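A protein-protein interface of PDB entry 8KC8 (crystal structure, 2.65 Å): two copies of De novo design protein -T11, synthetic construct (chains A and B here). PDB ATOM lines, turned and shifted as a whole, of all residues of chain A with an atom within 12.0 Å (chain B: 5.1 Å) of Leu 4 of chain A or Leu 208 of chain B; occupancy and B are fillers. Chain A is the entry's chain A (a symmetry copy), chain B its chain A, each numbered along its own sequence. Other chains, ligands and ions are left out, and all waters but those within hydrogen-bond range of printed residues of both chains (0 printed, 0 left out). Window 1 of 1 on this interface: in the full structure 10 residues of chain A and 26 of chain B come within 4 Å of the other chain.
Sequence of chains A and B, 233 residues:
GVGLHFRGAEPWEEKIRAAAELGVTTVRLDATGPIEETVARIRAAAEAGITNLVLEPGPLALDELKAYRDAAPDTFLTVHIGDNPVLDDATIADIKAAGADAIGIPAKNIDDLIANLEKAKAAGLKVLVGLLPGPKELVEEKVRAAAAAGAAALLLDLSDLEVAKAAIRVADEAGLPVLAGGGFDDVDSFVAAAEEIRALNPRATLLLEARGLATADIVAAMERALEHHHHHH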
ATOM      1  N   GLY A   1      -0.401  15.386  -8.134  1.00  0.00           N
ATOM      2  CA  GLY A   1      -0.714  14.001  -7.834  1.00  0.00           C
ATOM      3  C   GLY A   1      -2.187  13.778  -7.559  1.00  0.00           C
ATOM      4  O   GLY A   1      -2.808  14.529  -6.799  1.00  0.00           O
ATOM      5  N   VAL A   2      -2.746  12.746  -8.188  1.00  0.00           N
ATOM      6  CA  VAL A   2      -4.142  12.365  -8.015  1.00  0.00           C
ATOM      7  C   VAL A   2      -4.219  10.850  -7.874  1.00  0.00           C
ATOM      8  O   VAL A   2      -3.485  10.114  -8.547  1.00  0.00           O
ATOM      9  CB  VAL A   2      -5.018  12.848  -9.189  1.00  0.00           C
ATOM     10  CG1 VAL A   2      -5.156  14.357  -9.157  1.00  0.00           C
ATOM     11  CG2 VAL A   2      -4.431  12.395 -10.511  1.00  0.00           C
ATOM     12  N   GLY A   3      -5.113  10.386  -7.001  1.00  0.00           N
ATOM     13  CA  GLY A   3      -5.246   8.973  -6.709  1.00  0.00           C
ATOM     14  C   GLY A   3      -6.681   8.620  -6.373  1.00  0.00           C
ATOM     15  O   GLY A   3      -7.566   9.477  -6.345  1.00  0.00           O
ATOM     16  N   LEU A   4      -6.901   7.335  -6.112  1.00  0.00           N
ATOM     17  CA  LEU A   4      -8.219   6.800  -5.811  1.00  0.00           C
ATOM     18  C   LEU A   4      -8.306   6.423  -4.342  1.00  0.00           C
ATOM     19  O   LEU A   4      -7.359   5.870  -3.774  1.00  0.00           O
ATOM     20  CB  LEU A   4      -8.521   5.566  -6.658  1.00  0.00           C
ATOM     21  CG  LEU A   4      -8.693   5.811  -8.149  1.00  0.00           C
ATOM     22  CD1 LEU A   4      -9.278   4.574  -8.795  1.00  0.00           C
ATOM     23  CD2 LEU A   4      -9.575   7.028  -8.377  1.00  0.00           C
ATOM     24  N   HIS A   5      -9.448   6.716  -3.732  1.00  0.00           N
ATOM     25  CA  HIS A   5      -9.744   6.295  -2.369  1.00  0.00           C
ATOM     26  C   HIS A   5     -11.016   5.461  -2.393  1.00  0.00           C
ATOM     27  O   HIS A   5     -12.074   5.952  -2.805  1.00  0.00           O
ATOM     28  CB  HIS A   5      -9.908   7.500  -1.442  1.00  0.00           C
ATOM     29  CG  HIS A   5     -10.109   7.130  -0.006  1.00  0.00           C
ATOM     30  ND1 HIS A   5     -10.550   8.031   0.939  1.00  0.00           N
ATOM     31  CD2 HIS A   5      -9.918   5.958   0.649  1.00  0.00           C
ATOM     32  CE1 HIS A   5     -10.632   7.430   2.112  1.00  0.00           C
ATOM     33  NE2 HIS A   5     -10.251   6.173   1.965  1.00  0.00           N
ATOM     34  N   PHE A   6     -10.915   4.203  -1.969  1.00  0.00           N
ATOM     35  CA  PHE A   6     -12.074   3.319  -1.860  1.00  0.00           C
ATOM     36  C   PHE A   6     -12.409   3.198  -0.377  1.00  0.00           C
ATOM     37  O   PHE A   6     -11.935   2.297   0.314  1.00  0.00           O
ATOM     38  CB  PHE A   6     -11.798   1.964  -2.497  1.00  0.00           C
ATOM     39  CG  PHE A   6     -11.584   2.021  -3.987  1.00  0.00           C
ATOM     40  CD1 PHE A   6     -12.665   2.073  -4.852  1.00  0.00           C
ATOM     41  CD2 PHE A   6     -10.305   2.009  -4.522  1.00  0.00           C
ATOM     42  CE1 PHE A   6     -12.474   2.125  -6.224  1.00  0.00           C
ATOM     43  CE2 PHE A   6     -10.110   2.061  -5.892  1.00  0.00           C
ATOM     44  CZ  PHE A   6     -11.197   2.120  -6.742  1.00  0.00           C
ATOM     45  N   ARG A   7     -13.228   4.123   0.115  1.00  0.00           N
ATOM     46  CA  ARG A   7     -13.505   4.191   1.544  1.00  0.00           C
ATOM     47  C   ARG A   7     -14.471   3.090   1.958  1.00  0.00           C
ATOM     48  O   ARG A   7     -15.426   2.775   1.243  1.00  0.00           O
ATOM     49  CB  ARG A   7     -14.075   5.559   1.913  1.00  0.00           C
ATOM     50  CG  ARG A   7     -14.219   5.775   3.407  1.00  0.00           C
ATOM     51  CD  ARG A   7     -14.199   7.252   3.762  1.00  0.00           C
ATOM     52  NE  ARG A   7     -15.110   8.023   2.923  1.00  0.00           N
ATOM     53  CZ  ARG A   7     -16.418   8.121   3.126  1.00  0.00           C
ATOM     54  NH1 ARG A   7     -17.014   7.474   4.114  1.00  0.00           N
ATOM     55  NH2 ARG A   7     -17.146   8.890   2.321  1.00  0.00           N
ATOM     56  N   GLY A   8     -14.217   2.504   3.126  1.00  0.00           N
ATOM     57  CA  GLY A   8     -15.032   1.412   3.613  1.00  0.00           C
ATOM     58  C   GLY A   8     -16.275   1.886   4.344  1.00  0.00           C
ATOM     59  O   GLY A   8     -16.301   2.962   4.937  1.00  0.00           O
ATOM     60  N   LYS B  15     -12.447   0.321 -11.983  1.00  0.00           N
ATOM     61  CA  LYS B  15     -12.072   1.694 -11.665  1.00  0.00           C
ATOM     62  C   LYS B  15     -10.565   1.830 -11.485  1.00  0.00           C
ATOM     63  O   LYS B  15      -9.969   2.813 -11.939  1.00  0.00           O
ATOM     64  CB  LYS B  15     -12.818   2.154 -10.413  1.00  0.00           C
ATOM     65  CG  LYS B  15     -14.284   1.735 -10.382  1.00  0.00           C
ATOM     66  CD  LYS B  15     -15.098   2.638  -9.465  1.00  0.00           C
ATOM     67  CE  LYS B  15     -16.593   2.407  -9.629  1.00  0.00           C
ATOM     68  NZ  LYS B  15     -17.325   2.546  -8.337  1.00  0.00           N
ATOM     69  N   ILE B  16      -9.931   0.850 -10.838  1.00  0.00           N
ATOM     70  CA  ILE B  16      -8.484   0.900 -10.639  1.00  0.00           C
ATOM     71  C   ILE B  16      -7.762   0.875 -11.980  1.00  0.00           C
ATOM     72  O   ILE B  16      -6.839   1.660 -12.226  1.00  0.00           O
ATOM     73  CB  ILE B  16      -8.027  -0.260  -9.739  1.00  0.00           C
ATOM     74  CG1 ILE B  16      -8.418   0.013  -8.285  1.00  0.00           C
ATOM     75  CG2 ILE B  16      -6.520  -0.496  -9.899  1.00  0.00           C
ATOM     76  CD1 ILE B  16      -8.514  -1.236  -7.436  1.00  0.00           C
ATOM     77  N   ALA B  19      -8.207   4.233 -13.999  1.00  0.00           N
ATOM     78  CA  ALA B  19      -7.382   5.333 -13.508  1.00  0.00           C
ATOM     79  C   ALA B  19      -5.903   5.106 -13.810  1.00  0.00           C
ATOM     80  O   ALA B  19      -5.199   6.035 -14.227  1.00  0.00           O
ATOM     81  CB  ALA B  19      -7.609   5.526 -12.010  1.00  0.00           C
ATOM     82  N   VAL B  24      -2.478   7.129 -12.976  1.00  0.00           N
ATOM     83  CA  VAL B  24      -2.607   7.131 -11.524  1.00  0.00           C
ATOM     84  C   VAL B  24      -1.791   5.992 -10.925  1.00  0.00           C
ATOM     85  O   VAL B  24      -1.786   4.864 -11.442  1.00  0.00           O
ATOM     86  CB  VAL B  24      -4.085   7.035 -11.119  1.00  0.00           C
ATOM     87  CG1 VAL B  24      -4.226   7.209  -9.631  1.00  0.00           C
ATOM     88  CG2 VAL B  24      -4.888   8.099 -11.838  1.00  0.00           C
ATOM     89  N   THR B  26      -1.382   5.890  -7.094  1.00  0.00           N
ATOM     90  CA  THR B  26      -1.715   5.755  -5.680  1.00  0.00           C
ATOM     91  C   THR B  26      -3.179   5.370  -5.505  1.00  0.00           C
ATOM     92  O   THR B  26      -4.075   6.039  -6.035  1.00  0.00           O
ATOM     93  CB  THR B  26      -1.424   7.048  -4.915  1.00  0.00           C
ATOM     94  OG1 THR B  26      -0.065   7.440  -5.140  1.00  0.00           O
ATOM     95  CG2 THR B  26      -1.660   6.849  -3.422  1.00  0.00           C
ATOM     96  N   VAL B  27      -3.414   4.306  -4.743  1.00  0.00           N
ATOM     97  CA  VAL B  27      -4.754   3.857  -4.389  1.00  0.00           C
ATOM     98  C   VAL B  27      -4.797   3.622  -2.889  1.00  0.00           C
ATOM     99  O   VAL B  27      -3.927   2.936  -2.338  1.00  0.00           O
ATOM    100  CB  VAL B  27      -5.150   2.576  -5.145  1.00  0.00           C
ATOM    101  CG1 VAL B  27      -6.316   1.901  -4.457  1.00  0.00           C
ATOM    102  CG2 VAL B  27      -5.495   2.904  -6.590  1.00  0.00           C
ATOM    103  N   ARG B  28      -5.796   4.202  -2.230  1.00  0.00           N
ATOM    104  CA  ARG B  28      -6.075   3.942  -0.825  1.00  0.00           C
ATOM    105  C   ARG B  28      -7.255   2.978  -0.771  1.00  0.00           C
ATOM    106  O   ARG B  28      -8.371   3.326  -1.173  1.00  0.00           O
ATOM    107  CB  ARG B  28      -6.369   5.242  -0.084  1.00  0.00           C
ATOM    108  CG  ARG B  28      -6.542   5.093   1.412  1.00  0.00           C
ATOM    109  CD  ARG B  28      -6.601   6.458   2.067  1.00  0.00           C
ATOM    110  NE  ARG B  28      -7.275   6.407   3.358  1.00  0.00           N
ATOM    111  CZ  ARG B  28      -7.667   7.473   4.040  1.00  0.00           C
ATOM    112  NH1 ARG B  28      -7.442   8.701   3.597  1.00  0.00           N
ATOM    113  NH2 ARG B  28      -8.310   7.304   5.192  1.00  0.00           N
ATOM    114  N   PHE B 184     -14.401  14.652  -1.123  1.00  0.00           N
ATOM    115  CA  PHE B 184     -14.211  14.740  -2.570  1.00  0.00           C
ATOM    116  C   PHE B 184     -14.893  13.549  -3.236  1.00  0.00           C
ATOM    117  O   PHE B 184     -14.261  12.551  -3.580  1.00  0.00           O
ATOM    118  CB  PHE B 184     -12.732  14.799  -2.925  1.00  0.00           C
ATOM    119  CG  PHE B 184     -12.115  16.132  -2.670  1.00  0.00           C
ATOM    120  CD1 PHE B 184     -11.101  16.270  -1.740  1.00  0.00           C
ATOM    121  CD2 PHE B 184     -12.570  17.254  -3.336  1.00  0.00           C
ATOM    122  CE1 PHE B 184     -10.539  17.501  -1.492  1.00  0.00           C
ATOM    123  CE2 PHE B 184     -12.014  18.489  -3.093  1.00  0.00           C
ATOM    124  CZ  PHE B 184     -10.998  18.614  -2.166  1.00  0.00           C
ATOM    125  N   ASP B 186     -17.490  14.863  -5.531  1.00  0.00           N
ATOM    126  CA  ASP B 186     -17.911  15.663  -6.672  1.00  0.00           C
ATOM    127  C   ASP B 186     -16.746  15.834  -7.637  1.00  0.00           C
ATOM    128  O   ASP B 186     -15.601  16.031  -7.219  1.00  0.00           O
ATOM    129  CB  ASP B 186     -18.419  17.026  -6.196  1.00  0.00           C
ATOM    130  CG  ASP B 186     -18.875  17.926  -7.334  1.00  0.00           C
ATOM    131  OD1 ASP B 186     -19.003  17.458  -8.488  1.00  0.00           O
ATOM    132  OD2 ASP B 186     -19.098  19.124  -7.064  1.00  0.00           O
ATOM    133  N   PHE B 190     -13.331  18.473  -7.071  1.00  0.00           N
ATOM    134  CA  PHE B 190     -12.063  17.765  -6.944  1.00  0.00           C
ATOM    135  C   PHE B 190     -11.000  18.370  -7.854  1.00  0.00           C
ATOM    136  O   PHE B 190      -9.874  18.636  -7.416  1.00  0.00           O
ATOM    137  CB  PHE B 190     -12.259  16.278  -7.255  1.00  0.00           C
ATOM    138  CG  PHE B 190     -10.985  15.565  -7.622  1.00  0.00           C
ATOM    139  CD1 PHE B 190     -10.138  15.083  -6.635  1.00  0.00           C
ATOM    140  CD2 PHE B 190     -10.628  15.386  -8.951  1.00  0.00           C
ATOM    141  CE1 PHE B 190      -8.960  14.436  -6.965  1.00  0.00           C
ATOM    142  CE2 PHE B 190      -9.450  14.744  -9.285  1.00  0.00           C
ATOM    143  CZ  PHE B 190      -8.615  14.272  -8.290  1.00  0.00           C
ATOM    144  N   LEU B 206      -3.784  14.186  -4.129  1.00  0.00           N
ATOM    145  CA  LEU B 206      -5.179  14.325  -3.742  1.00  0.00           C
ATOM    146  C   LEU B 206      -5.939  13.077  -4.174  1.00  0.00           C
ATOM    147  O   LEU B 206      -5.803  12.622  -5.315  1.00  0.00           O
ATOM    148  CB  LEU B 206      -5.792  15.578  -4.370  1.00  0.00           C
ATOM    149  CG  LEU B 206      -7.165  16.016  -3.859  1.00  0.00           C
ATOM    150  CD1 LEU B 206      -7.123  16.355  -2.374  1.00  0.00           C
ATOM    151  CD2 LEU B 206      -7.669  17.200  -4.666  1.00  0.00           C
ATOM    152  N   LEU B 207      -6.734  12.529  -3.265  1.00  0.00           N
ATOM    153  CA  LEU B 207      -7.455  11.289  -3.508  1.00  0.00           C
ATOM    154  C   LEU B 207      -8.908  11.592  -3.839  1.00  0.00           C
ATOM    155  O   LEU B 207      -9.574  12.336  -3.112  1.00  0.00           O
ATOM    156  CB  LEU B 207      -7.366  10.375  -2.289  1.00  0.00           C
ATOM    157  CG  LEU B 207      -5.942   9.994  -1.892  1.00  0.00           C
ATOM    158  CD1 LEU B 207      -5.976   9.154  -0.638  1.00  0.00           C
ATOM    159  CD2 LEU B 207      -5.262   9.237  -3.037  1.00  0.00           C
ATOM    160  N   LEU B 208      -9.379  11.039  -4.957  1.00  0.00           N
ATOM    161  CA  LEU B 208     -10.796  11.035  -5.304  1.00  0.00           C
ATOM    162  C   LEU B 208     -11.494   9.851  -4.644  1.00  0.00           C
ATOM    163  O   LEU B 208     -11.073   8.701  -4.811  1.00  0.00           O
ATOM    164  CB  LEU B 208     -10.985  10.975  -6.822  1.00  0.00           C
ATOM    165  CG  LEU B 208     -12.405  11.196  -7.364  1.00  0.00           C
ATOM    166  CD1 LEU B 208     -12.731  12.675  -7.581  1.00  0.00           C
ATOM    167  CD2 LEU B 208     -12.594  10.419  -8.664  1.00  0.00           C
ATOM    168  N   GLU B 209     -12.561  10.132  -3.899  1.00  0.00           N
ATOM    169  CA  GLU B 209     -13.412   9.064  -3.386  1.00  0.00           C
ATOM    170  C   GLU B 209     -14.145   8.421  -4.560  1.00  0.00           C
ATOM    171  O   GLU B 209     -15.011   9.047  -5.180  1.00  0.00           O
ATOM    172  CB  GLU B 209     -14.387   9.611  -2.349  1.00  0.00           C
ATOM    173  CG  GLU B 209     -13.730  10.095  -1.057  1.00  0.00           C
ATOM    174  CD  GLU B 209     -14.721  10.228   0.093  1.00  0.00           C
ATOM    175  OE1 GLU B 209     -15.779   9.562   0.050  1.00  0.00           O
ATOM    176  OE2 GLU B 209     -14.450  11.004   1.035  1.00  0.00           O
ATOM    177  N   ALA B 210     -13.794   7.172  -4.876  1.00  0.00           N
ATOM    178  CA  ALA B 210     -14.229   6.511  -6.100  1.00  0.00           C
ATOM    179  C   ALA B 210     -15.271   5.429  -5.858  1.00  0.00           C
ATOM    180  O   ALA B 210     -15.669   4.743  -6.807  1.00  0.00           O
ATOM    181  CB  ALA B 210     -13.022   5.907  -6.826  1.00  0.00           C
ATOM    182  N   LEU B 213     -18.740   6.676  -7.662  1.00  0.00           N
ATOM    183  CA  LEU B 213     -18.710   7.322  -8.966  1.00  0.00           C
ATOM    184  C   LEU B 213     -18.626   6.288 -10.082  1.00  0.00           C
ATOM    185  O   LEU B 213     -18.063   5.202  -9.912  1.00  0.00           O
ATOM    186  CB  LEU B 213     -17.525   8.283  -9.067  1.00  0.00           C
ATOM    187  CG  LEU B 213     -17.786   9.750  -8.738  1.00  0.00           C
ATOM    188  CD1 LEU B 213     -18.229   9.891  -7.294  1.00  0.00           C
ATOM    189  CD2 LEU B 213     -16.541  10.586  -9.005  1.00  0.00           C
ATOM    190  N   ILE B 218     -14.887   8.918 -13.253  1.00  0.00           N
ATOM    191  CA  ILE B 218     -13.541   8.875 -12.692  1.00  0.00           C
ATOM    192  C   ILE B 218     -12.519   9.213 -13.765  1.00  0.00           C
ATOM    193  O   ILE B 218     -11.587   9.989 -13.530  1.00  0.00           O
ATOM    194  CB  ILE B 218     -13.259   7.501 -12.059  1.00  0.00           C
ATOM    195  CG1 ILE B 218     -14.152   7.268 -10.848  1.00  0.00           C
ATOM    196  CG2 ILE B 218     -11.814   7.401 -11.632  1.00  0.00           C
ATOM    197  CD1 ILE B 218     -14.036   5.878 -10.307  1.00  0.00           C
ATOM    198  N   ALA B 221     -12.653  12.840 -14.286  1.00  0.00           N
ATOM    199  CA  ALA B 221     -12.003  13.553 -13.192  1.00  0.00           C
ATOM    200  C   ALA B 221     -10.485  13.464 -13.291  1.00  0.00           C
ATOM    201  O   ALA B 221      -9.790  14.469 -13.106  1.00  0.00           O
ATOM    202  CB  ALA B 221     -12.483  13.006 -11.848  1.00  0.00           C
ATOM    203  N   MET B 222      -9.950  12.277 -13.586  1.00  0.00           N
ATOM    204  CA  MET B 222      -8.497  12.132 -13.633  1.00  0.00           C
ATOM    205  C   MET B 222      -7.906  12.826 -14.853  1.00  0.00           C
ATOM    206  O   MET B 222      -6.799  13.374 -14.778  1.00  0.00           O
ATOM    207  CB  MET B 222      -8.095  10.657 -13.614  1.00  0.00           C
ATOM    208  CG  MET B 222      -8.640   9.817 -12.452  1.00  0.00           C
ATOM    209  SD  MET B 222      -7.801   9.936 -10.852  1.00  0.00           S
ATOM    210  CE  MET B 222      -8.328  11.513 -10.208  1.00  0.00           C
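O of Arg 28 of chain B sits at hydrogen-bond distance from N of Phe 6 of chain A (2.8 Å).
O of His 5 of chain A is in hydrogen-bond range of N of Ala 210 of chain B, at 3.0 Å.
The backbone carbonyl oxygen of Leu 208 of chain B is in hydrogen-bond range of the backbone NH of His 5 of chain A, at 2.8 Å.
N of Arg 28 of chain B is in hydrogen-bond range of O of Leu 4 of chain A, 2.8 Å away.
The backbone NH of Leu 208 of chain B is in hydrogen-bond range of the backbone carbonyl oxygen of Gly 3 of chain A (2.8 Å).
O of Gly 1 of chain A lies within hydrogen-bond range of N of Leu 206 of chain B (2.9 Å).
The backbone carbonyl oxygen (O) of Thr 26 of chain B is in hydrogen-bond range of the backbone NH (N) of Leu 4 of chain A (3.1 Å).
The guanidinium group (NH2) of Arg 7 of chain A lies within salt-bridge range of the side-chain carboxylate (OE1) of Glu 209 of chain B (2.7 Å).
The backbone NH (N) of Gly 3 of chain A lies within hydrogen-bond range of the backbone carbonyl oxygen (O) of Leu 206 of chain B.
The guanidinium group (NE) of Arg 28 of chain B is in hydrogen-bond range of a ring nitrogen (NE2) of His 5 of chain A.
The backbone carbonyl oxygen (O) of Phe 184 of chain B is in hydrogen-bond range of the backbone NH (N) of Glu 209 of chain B (3.0 Å).
The backbone carbonyl oxygen (O) of Ala 19 of chain B lies close to the backbone NH (N) of Val 24 of chain B.
The side-chain amino group of Lys 15 of chain B sits at hydrogen-bond distance from the backbone carbonyl oxygen of Ala 210 of chain B (3.1 Å).
O of Leu 213 of chain B lies close to NZ of Lys 15 of chain B, 3.2 Å away.
Among the printed residues, pairs that only touch across the chains: Val 2 of chain A with Val 24 of chain B (3.2 Å), Val 2 of chain A with Phe 190 of chain B (3.6 Å), Val 2 of chain A with Leu 206 of chain B (3.2 Å), Val 2 of chain A with Met 222 of chain B (3.7 Å), Gly 3 of chain A with Val 24 of chain B (3.6 Å), Gly 3 of chain A with Thr 26 of chain B (3.2 Å), Gly 3 of chain A with Leu 207 of chain B (3.4 Å), Leu 4 of chain A with Lys 15 of chain B (3.7 Å), Leu 4 of chain A with Ala 19 of chain B (3.7 Å), Leu 4 of chain A with Val 27 of chain B (3.3 Å), Leu 4 of chain A with Leu 207 of chain B (3.97 Å), Leu 4 of chain A with Leu 208 of chain B (3.6 Å), Leu 4 of chain A with Ala 210 of chain B (3.9 Å), Leu 4 of chain A with Ile 218 of chain B (3.97 Å), His 5 of chain A with Leu 207 of chain B (3.9 Å), His 5 of chain A with Glu 209 of chain B (3.4 Å), Phe 6 of chain A with Ile 16 of chain B (3.6 Å), Phe 6 of chain A with Val 27 of chain B (3.99 Å) and Phe 6 of chain A with Ala 210 of chain B (3.9 Å).
Leu 4 of chain A touches just these residues of chain B: Lys 15 (3.7 Å), Ala 19 (3.7 Å), Thr 26 (3.1 Å), Val 27 (3.3 Å), Arg 28 (2.8 Å), Leu 207 (3.97 Å), Leu 208 (3.6 Å), Ala 210 (3.9 Å) and Ile 218 (3.97 Å).
Of chain A, only Gly 3 (2.8 Å), Leu 4 (3.6 Å) and His 5 (2.8 Å) come within 4 Å of Leu 208 of chain B.
Of the printed residues of chain A, Ile 16 of chain B touches Phe 6 (3.6 Å).
Ala 19 of chain B touches just one residue of chain A: Leu 4 (3.7 Å).
Of chain A, only Val 2 comes within 4 Å of Phe 190 of chain B.
Leu 206 of chain B touches just these residues of chain A: Gly 1 (2.9 Å), Val 2 (3.2 Å) and Gly 3 (2.9 Å).
Of chain A, only Gly 3, Leu 4 and His 5 come within 4 Å of Leu 207 of chain B.
Of chain A, only Leu 4 (3.97 Å) comes within 4 Å of Ile 218 of chain B.
No residue of chain A comes within 4 Å of Ala 221 of chain B.
Printed residues of chain A within 4 Å of Val 24 of chain B: Val 2 and Gly 3.
Of the printed residues of chain B, Gly 1 of chain A touches Leu 206.
Printed residues of chain B within 4 Å of Gly 3 of chain A: Val 24 (3.6 Å), Thr 26 (3.2 Å), Leu 206 (2.9 Å), Leu 207 (3.4 Å) and Leu 208 (2.8 Å).
Of the printed residues of chain B, His 5 of chain A touches Arg 28, Leu 207, Leu 208, Glu 209 and Ala 210.
Asp 186 of chain B touches none of the printed residues of chain A.
The nearest printed residue of chain B that does not touch Leu 4 of chain A is Ile 16 of chain B (4.2 Å).
The nearest residue of chain A that does not touch Leu 208 of chain B is Phe 6 of chain A (5.3 Å).
The nearest printed residue of chain B that does not touch His 5 of chain A is Val 27 of chain B (5.5 Å).
Of the 19 printed residues of chain B, 15 touch a printed residue of chain A.
Hydrophobic or aromatic side chains of chain B that line the printed part of chain A: Ile 16, Ala 19, Val 24, Val 27, Phe 190, Leu 206, Leu 207, Leu 208, Ala 210, Ile 218 and Met 222.
Printed residues of chain A that touch a printed residue of chain B: Gly 1, Val 2, Gly 3, Leu 4, His 5, Phe 6 and Arg 7.
Hydrophobic or aromatic side chains of chain A within 4 Å of the printed part of chain B: Val 2, Leu 4, His 5 and Phe 6.
No position is printed for both chains.
Of the 29 pairs that touch across the chains among the printed residues, none has its exchanged pair printed and touching as well.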
